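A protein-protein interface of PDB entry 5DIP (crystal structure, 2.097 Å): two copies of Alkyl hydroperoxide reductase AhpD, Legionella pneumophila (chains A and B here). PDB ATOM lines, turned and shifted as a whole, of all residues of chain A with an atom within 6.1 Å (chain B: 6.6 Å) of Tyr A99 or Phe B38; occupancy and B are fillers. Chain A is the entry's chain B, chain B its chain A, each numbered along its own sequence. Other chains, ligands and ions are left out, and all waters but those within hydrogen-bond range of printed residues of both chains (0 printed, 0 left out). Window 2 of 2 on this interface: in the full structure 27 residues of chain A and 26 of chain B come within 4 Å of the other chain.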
ATOM      1  N   LEU A  94       7.150  11.141   0.100  1.00  0.00           N
ATOM      2  CA  LEU A  94       5.804  11.126   0.647  1.00  0.00           C
ATOM      3  C   LEU A  94       5.572   9.835   1.451  1.00  0.00           C
ATOM      4  O   LEU A  94       4.940   9.862   2.494  1.00  0.00           O
ATOM      5  CB  LEU A  94       4.762  11.244  -0.470  1.00  0.00           C
ATOM      6  CG  LEU A  94       4.828  12.542  -1.281  1.00  0.00           C
ATOM      7  CD1 LEU A  94       3.729  12.563  -2.338  1.00  0.00           C
ATOM      8  CD2 LEU A  94       4.745  13.768  -0.355  1.00  0.00           C
ATOM      9  N   GLY A  95       6.074   8.720   0.938  1.00  0.00           N
ATOM     10  CA  GLY A  95       6.034   7.459   1.661  1.00  0.00           C
ATOM     11  C   GLY A  95       6.602   7.603   3.069  1.00  0.00           C
ATOM     12  O   GLY A  95       6.034   7.093   4.031  1.00  0.00           O
ATOM     13  N   MET A  96       7.717   8.320   3.197  1.00  0.00           N
ATOM     14  CA  MET A  96       8.316   8.511   4.508  1.00  0.00           C
ATOM     15  C   MET A  96       7.413   9.353   5.401  1.00  0.00           C
ATOM     16  O   MET A  96       7.288   9.071   6.587  1.00  0.00           O
ATOM     17  CB  MET A  96       9.703   9.151   4.388  1.00  0.00           C
ATOM     18  CG  MET A  96      10.761   8.193   3.814  1.00  0.00           C
ATOM     19  SD  MET A  96      10.999   6.715   4.844  1.00  0.00           S
ATOM     20  CE  MET A  96      11.442   7.459   6.412  1.00  0.00           C
ATOM     21  N   ALA A  97       6.788  10.386   4.841  1.00  0.00           N
ATOM     22  CA  ALA A  97       5.858  11.199   5.620  1.00  0.00           C
ATOM     23  C   ALA A  97       4.660  10.364   6.116  1.00  0.00           C
ATOM     24  O   ALA A  97       4.178  10.564   7.228  1.00  0.00           O
ATOM     25  CB  ALA A  97       5.375  12.386   4.798  1.00  0.00           C
ATOM     26  N   VAL A  98       4.187   9.432   5.290  1.00  0.00           N
ATOM     27  CA  VAL A  98       3.033   8.610   5.672  1.00  0.00           C
ATOM     28  C   VAL A  98       3.407   7.638   6.800  1.00  0.00           C
ATOM     29  O   VAL A  98       2.671   7.477   7.765  1.00  0.00           O
ATOM     30  CB  VAL A  98       2.466   7.829   4.465  1.00  0.00           C
ATOM     31  CG1 VAL A  98       1.350   6.877   4.923  1.00  0.00           C
ATOM     32  CG2 VAL A  98       1.942   8.799   3.410  1.00  0.00           C
ATOM     33  N   TYR A  99       4.566   7.007   6.673  1.00  0.00           N
ATOM     34  CA  TYR A  99       5.106   6.168   7.740  1.00  0.00           C
ATOM     35  C   TYR A  99       5.223   6.932   9.070  1.00  0.00           C
ATOM     36  O   TYR A  99       4.936   6.392  10.138  1.00  0.00           O
ATOM     37  CB  TYR A  99       6.455   5.603   7.279  1.00  0.00           C
ATOM     38  CG  TYR A  99       7.442   5.169   8.341  1.00  0.00           C
ATOM     39  CD1 TYR A  99       7.074   4.322   9.382  1.00  0.00           C
ATOM     40  CD2 TYR A  99       8.772   5.562   8.257  1.00  0.00           C
ATOM     41  CE1 TYR A  99       8.008   3.918  10.339  1.00  0.00           C
ATOM     42  CE2 TYR A  99       9.700   5.165   9.195  1.00  0.00           C
ATOM     43  CZ  TYR A  99       9.321   4.346  10.232  1.00  0.00           C
ATOM     44  OH  TYR A  99      10.272   3.960  11.157  1.00  0.00           O
ATOM     45  N   MET A 100       5.593   8.203   9.018  1.00  0.00           N
ATOM     46  CA  MET A 100       5.784   9.017  10.210  1.00  0.00           C
ATOM     47  C   MET A 100       4.589   9.896  10.560  1.00  0.00           C
ATOM     48  O   MET A 100       4.699  10.769  11.411  1.00  0.00           O
ATOM     49  CB  MET A 100       7.015   9.910  10.038  1.00  0.00           C
ATOM     50  CG  MET A 100       8.150   9.216   9.332  1.00  0.00           C
ATOM     51  SD  MET A 100       9.671   9.218  10.260  1.00  0.00           S
ATOM     52  CE  MET A 100       9.029   8.541  11.783  1.00  0.00           C
ATOM     53  N   GLY A 101       3.458   9.707   9.893  1.00  0.00           N
ATOM     54  CA  GLY A 101       2.324  10.581  10.174  1.00  0.00           C
ATOM     55  C   GLY A 101       0.967   9.899  10.118  1.00  0.00           C
ATOM     56  O   GLY A 101      -0.042  10.461  10.560  1.00  0.00           O
ATOM     57  N   GLY A 102       0.934   8.692   9.564  1.00  0.00           N
ATOM     58  CA  GLY A 102      -0.306   7.947   9.483  1.00  0.00           C
ATOM     59  C   GLY A 102      -1.348   8.596   8.587  1.00  0.00           C
ATOM     60  O   GLY A 102      -1.011   9.332   7.660  1.00  0.00           O
ATOM     61  N   GLU B  33      -1.892  -8.235  14.581  1.00  0.00           N
ATOM     62  CA  GLU B  33      -2.316  -7.804  13.248  1.00  0.00           C
ATOM     63  C   GLU B  33      -1.905  -6.348  12.992  1.00  0.00           C
ATOM     64  O   GLU B  33      -1.398  -6.004  11.934  1.00  0.00           O
ATOM     65  CB  GLU B  33      -3.832  -7.954  13.057  1.00  0.00           C
ATOM     66  CG  GLU B  33      -4.249  -7.800  11.577  1.00  0.00           C
ATOM     67  CD  GLU B  33      -5.764  -7.667  11.371  1.00  0.00           C
ATOM     68  OE1 GLU B  33      -6.190  -7.299  10.248  1.00  0.00           O
ATOM     69  OE2 GLU B  33      -6.522  -7.930  12.326  1.00  0.00           O
ATOM     70  N   LEU B  34      -2.163  -5.505  13.980  1.00  0.00           N
ATOM     71  CA  LEU B  34      -1.820  -4.087  13.921  1.00  0.00           C
ATOM     72  C   LEU B  34      -0.323  -3.877  13.690  1.00  0.00           C
ATOM     73  O   LEU B  34       0.080  -3.127  12.795  1.00  0.00           O
ATOM     74  CB  LEU B  34      -2.265  -3.426  15.226  1.00  0.00           C
ATOM     75  CG  LEU B  34      -2.386  -1.940  15.599  1.00  0.00           C
ATOM     76  CD1 LEU B  34      -1.062  -1.285  15.840  1.00  0.00           C
ATOM     77  CD2 LEU B  34      -3.217  -1.161  14.624  1.00  0.00           C
ATOM     78  N   MET B  35       0.497  -4.538  14.501  1.00  0.00           N
ATOM     79  CA  MET B  35       1.944  -4.361  14.414  1.00  0.00           C
ATOM     80  C   MET B  35       2.513  -4.983  13.142  1.00  0.00           C
ATOM     81  O   MET B  35       3.512  -4.502  12.611  1.00  0.00           O
ATOM     82  CB  MET B  35       2.624  -4.947  15.645  1.00  0.00           C
ATOM     83  CG  MET B  35       2.278  -4.196  16.934  1.00  0.00           C
ATOM     84  SD  MET B  35       2.718  -2.446  16.820  1.00  0.00           S
ATOM     85  CE  MET B  35       4.501  -2.570  16.816  1.00  0.00           C
ATOM     86  N   THR B  36       1.884  -6.048  12.649  1.00  0.00           N
ATOM     87  CA  THR B  36       2.292  -6.605  11.357  1.00  0.00           C
ATOM     88  C   THR B  36       2.026  -5.591  10.245  1.00  0.00           C
ATOM     89  O   THR B  36       2.861  -5.386   9.363  1.00  0.00           O
ATOM     90  CB  THR B  36       1.562  -7.938  11.048  1.00  0.00           C
ATOM     91  OG1 THR B  36       1.955  -8.914  12.022  1.00  0.00           O
ATOM     92  CG2 THR B  36       1.935  -8.454   9.663  1.00  0.00           C
ATOM     93  N   GLY B  37       0.860  -4.951  10.305  1.00  0.00           N
ATOM     94  CA  GLY B  37       0.503  -3.933   9.336  1.00  0.00           C
ATOM     95  C   GLY B  37       1.477  -2.769   9.429  1.00  0.00           C
ATOM     96  O   GLY B  37       1.984  -2.288   8.416  1.00  0.00           O
ATOM     97  N   PHE B  38       1.752  -2.324  10.649  1.00  0.00           N
ATOM     98  CA  PHE B  38       2.678  -1.209  10.828  1.00  0.00           C
ATOM     99  C   PHE B  38       4.070  -1.556  10.301  1.00  0.00           C
ATOM    100  O   PHE B  38       4.710  -0.743   9.634  1.00  0.00           O
ATOM    101  CB  PHE B  38       2.788  -0.790  12.294  1.00  0.00           C
ATOM    102  CG  PHE B  38       3.657   0.418  12.486  1.00  0.00           C
ATOM    103  CD1 PHE B  38       3.132   1.688  12.330  1.00  0.00           C
ATOM    104  CD2 PHE B  38       5.013   0.286  12.759  1.00  0.00           C
ATOM    105  CE1 PHE B  38       3.941   2.817  12.467  1.00  0.00           C
ATOM    106  CE2 PHE B  38       5.825   1.413  12.893  1.00  0.00           C
ATOM    107  CZ  PHE B  38       5.286   2.670  12.752  1.00  0.00           C
ATOM    108  N   SER B  39       4.531  -2.760  10.619  1.00  0.00           N
ATOM    109  CA  SER B  39       5.839  -3.220  10.168  1.00  0.00           C
ATOM    110  C   SER B  39       5.938  -3.227   8.644  1.00  0.00           C
ATOM    111  O   SER B  39       6.969  -2.860   8.085  1.00  0.00           O
ATOM    112  CB  SER B  39       6.131  -4.618  10.713  1.00  0.00           C
ATOM    113  OG  SER B  39       7.317  -5.131  10.140  1.00  0.00           O
ATOM    114  N   SER B  40       4.865  -3.644   7.978  1.00  0.00           N
ATOM    115  CA  SER B  40       4.820  -3.647   6.516  1.00  0.00           C
ATOM    116  C   SER B  40       4.911  -2.221   5.963  1.00  0.00           C
ATOM    117  O   SER B  40       5.641  -1.955   5.006  1.00  0.00           O
ATOM    118  CB  SER B  40       3.543  -4.320   6.010  1.00  0.00           C
ATOM    119  OG  SER B  40       3.580  -5.710   6.268  1.00  0.00           O
ATOM    120  N   LEU B  41       4.168  -1.312   6.580  1.00  0.00           N
ATOM    121  CA  LEU B  41       4.216   0.090   6.193  1.00  0.00           C
ATOM    122  C   LEU B  41       5.633   0.644   6.324  1.00  0.00           C
ATOM    123  O   LEU B  41       6.158   1.260   5.406  1.00  0.00           O
ATOM    124  CB  LEU B  41       3.250   0.902   7.056  1.00  0.00           C
ATOM    125  CG  LEU B  41       3.304   2.424   6.888  1.00  0.00           C
ATOM    126  CD1 LEU B  41       2.952   2.820   5.471  1.00  0.00           C
ATOM    127  CD2 LEU B  41       2.349   3.098   7.885  1.00  0.00           C
ATOM    128  N   ALA B  42       6.236   0.412   7.486  1.00  0.00           N
ATOM    129  CA  ALA B  42       7.559   0.935   7.787  1.00  0.00           C
ATOM    130  C   ALA B  42       8.603   0.375   6.815  1.00  0.00           C
ATOM    131  O   ALA B  42       9.457   1.107   6.314  1.00  0.00           O
ATOM    132  CB  ALA B  42       7.943   0.605   9.236  1.00  0.00           C
ATOM    133  N   GLN B  43       8.520  -0.923   6.539  1.00  0.00           N
ATOM    134  CA  GLN B  43       9.511  -1.559   5.685  1.00  0.00           C
ATOM    135  C   GLN B  43       9.372  -1.086   4.238  1.00  0.00           C
ATOM    136  O   GLN B  43      10.366  -0.860   3.557  1.00  0.00           O
ATOM    137  CB  GLN B  43       9.393  -3.080   5.771  1.00  0.00           C
ATOM    138  CG  GLN B  43       9.880  -3.783   4.524  1.00  0.00           C
ATOM    139  CD  GLN B  43      10.338  -5.198   4.796  1.00  0.00           C
ATOM    140  OE1 GLN B  43       9.546  -6.141   4.749  1.00  0.00           O
ATOM    141  NE2 GLN B  43      11.630  -5.356   5.083  1.00  0.00           N
ATOM    142  N   ALA B  45       8.228   1.830   3.364  1.00  0.00           N
ATOM    143  CA  ALA B  45       8.597   3.240   3.317  1.00  0.00           C
ATOM    144  C   ALA B  45      10.118   3.431   3.272  1.00  0.00           C
ATOM    145  O   ALA B  45      10.612   4.347   2.623  1.00  0.00           O
ATOM    146  CB  ALA B  45       8.017   3.991   4.523  1.00  0.00           C
ATOM    147  N   THR B  46      10.844   2.563   3.967  1.00  0.00           N
ATOM    148  CA  THR B  46      12.274   2.756   4.187  1.00  0.00           C
ATOM    149  C   THR B  46      13.175   1.934   3.267  1.00  0.00           C
ATOM    150  O   THR B  46      14.391   2.117   3.264  1.00  0.00           O
ATOM    151  CB  THR B  46      12.647   2.429   5.639  1.00  0.00           C
ATOM    152  OG1 THR B  46      12.266   1.079   5.931  1.00  0.00           O
ATOM    153  CG2 THR B  46      11.914   3.367   6.597  1.00  0.00           C
ATOM    154  N   GLU B  57      16.361   7.667   5.683  1.00  0.00           N
ATOM    155  CA  GLU B  57      16.539   7.823   7.125  1.00  0.00           C
ATOM    156  C   GLU B  57      16.898   9.255   7.513  1.00  0.00           C
ATOM    157  O   GLU B  57      16.599   9.688   8.616  1.00  0.00           O
ATOM    158  CB  GLU B  57      17.609   6.867   7.655  1.00  0.00           C
ATOM    159  CG  GLU B  57      17.114   5.438   7.856  1.00  0.00           C
ATOM    160  CD  GLU B  57      15.999   5.319   8.889  1.00  0.00           C
ATOM    161  OE1 GLU B  57      15.990   6.070   9.900  1.00  0.00           O
ATOM    162  OE2 GLU B  57      15.134   4.451   8.692  1.00  0.00           O
ATOM    163  N   ALA B  60      13.658  10.755   7.612  1.00  0.00           N
ATOM    164  CA  ALA B  60      13.028  10.359   8.876  1.00  0.00           C
ATOM    165  C   ALA B  60      13.541  11.191  10.037  1.00  0.00           C
ATOM    166  O   ALA B  60      12.771  11.559  10.919  1.00  0.00           O
ATOM    167  CB  ALA B  60      13.261   8.878   9.161  1.00  0.00           C
ATOM    168  N   HIS B  76      15.978   6.780  14.967  1.00  0.00           N
ATOM    169  CA  HIS B  76      16.476   7.104  13.642  1.00  0.00           C
ATOM    170  C   HIS B  76      17.941   7.562  13.671  1.00  0.00           C
ATOM    171  O   HIS B  76      18.666   7.337  12.712  1.00  0.00           O
ATOM    172  CB  HIS B  76      15.553   8.125  12.982  1.00  0.00           C
ATOM    173  CG  HIS B  76      14.195   7.560  12.681  1.00  0.00           C
ATOM    174  ND1 HIS B  76      14.005   6.526  11.786  1.00  0.00           N
ATOM    175  CD2 HIS B  76      12.973   7.846  13.188  1.00  0.00           C
ATOM    176  CE1 HIS B  76      12.721   6.208  11.748  1.00  0.00           C
ATOM    177  NE2 HIS B  76      12.072   7.002  12.582  1.00  0.00           N
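The side-chain sulfur (SD) of Met A96 lies close to the backbone carbonyl oxygen (O) of Ala B45, 3.3 Å away.
The side-chain carboxylate of Glu B57 sits at hydrogen-bond distance from a ring nitrogen (ND1) of His B76 (2.8 Å).
O of Ala B42 is in hydrogen-bond range of OG1 of Thr B46 (2.8 Å).
Among the printed residues, pairs that only touch across the chains: Tyr A99 with His B76 (3.4 Å), Tyr A99 with Ala B42 (3.5 Å), Met A100 with His B76 (3.5 Å), Tyr A99 with Ala B45 (3.6 Å), Met A96 with Ala B60 (3.6 Å), Gly A95 with Ala B45 (3.7 Å), Met A100 with Ala B60 (3.8 Å), Tyr A99 with Phe B38 (3.8 Å), Tyr A99 with Thr B46 (3.9 Å) and Met A96 with Thr B46 (3.9 Å).
Tyr A99 touches five residues of chain B.
Phe B38 touches just one residue of chain A: Tyr A99 (3.8 Å).
Printed residues of chain A within 4 Å of Ala B42: Tyr A99 (3.5 Å).
Of the printed residues of chain A, Thr B46 touches Met A96 and Tyr A99.
Printed residues of chain A within 4 Å of Ala B60: Met A96 and Met A100.
Of the printed residues of chain B, Gly A95 touches Ala B45 (3.7 Å).
Gly A102 touches none of the printed residues of chain B.
Leu B34 touches none of the printed residues of chain A.
The nearest printed residue of chain A that does not touch Phe B38 is Met A100 (6.6 Å).
Printed residues of chain B that touch a printed residue of chain A: Phe B38, Ala B42, Ala B45, Thr B46, Ala B60 and His B76.
Of the 9 printed residues of chain A, 4 touch a printed residue of chain B.
Among the printed residues, 11 pairs touch across the chains.
Among the printed residues, no Asp or Glu carboxylate lies within 4 Å of a Lys or Arg side-chain nitrogen of the other chain.
No position is printed for both chains.
Of the 11 pairs that touch across the chains among the printed residues, none has its exchanged pair printed and touching as well.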
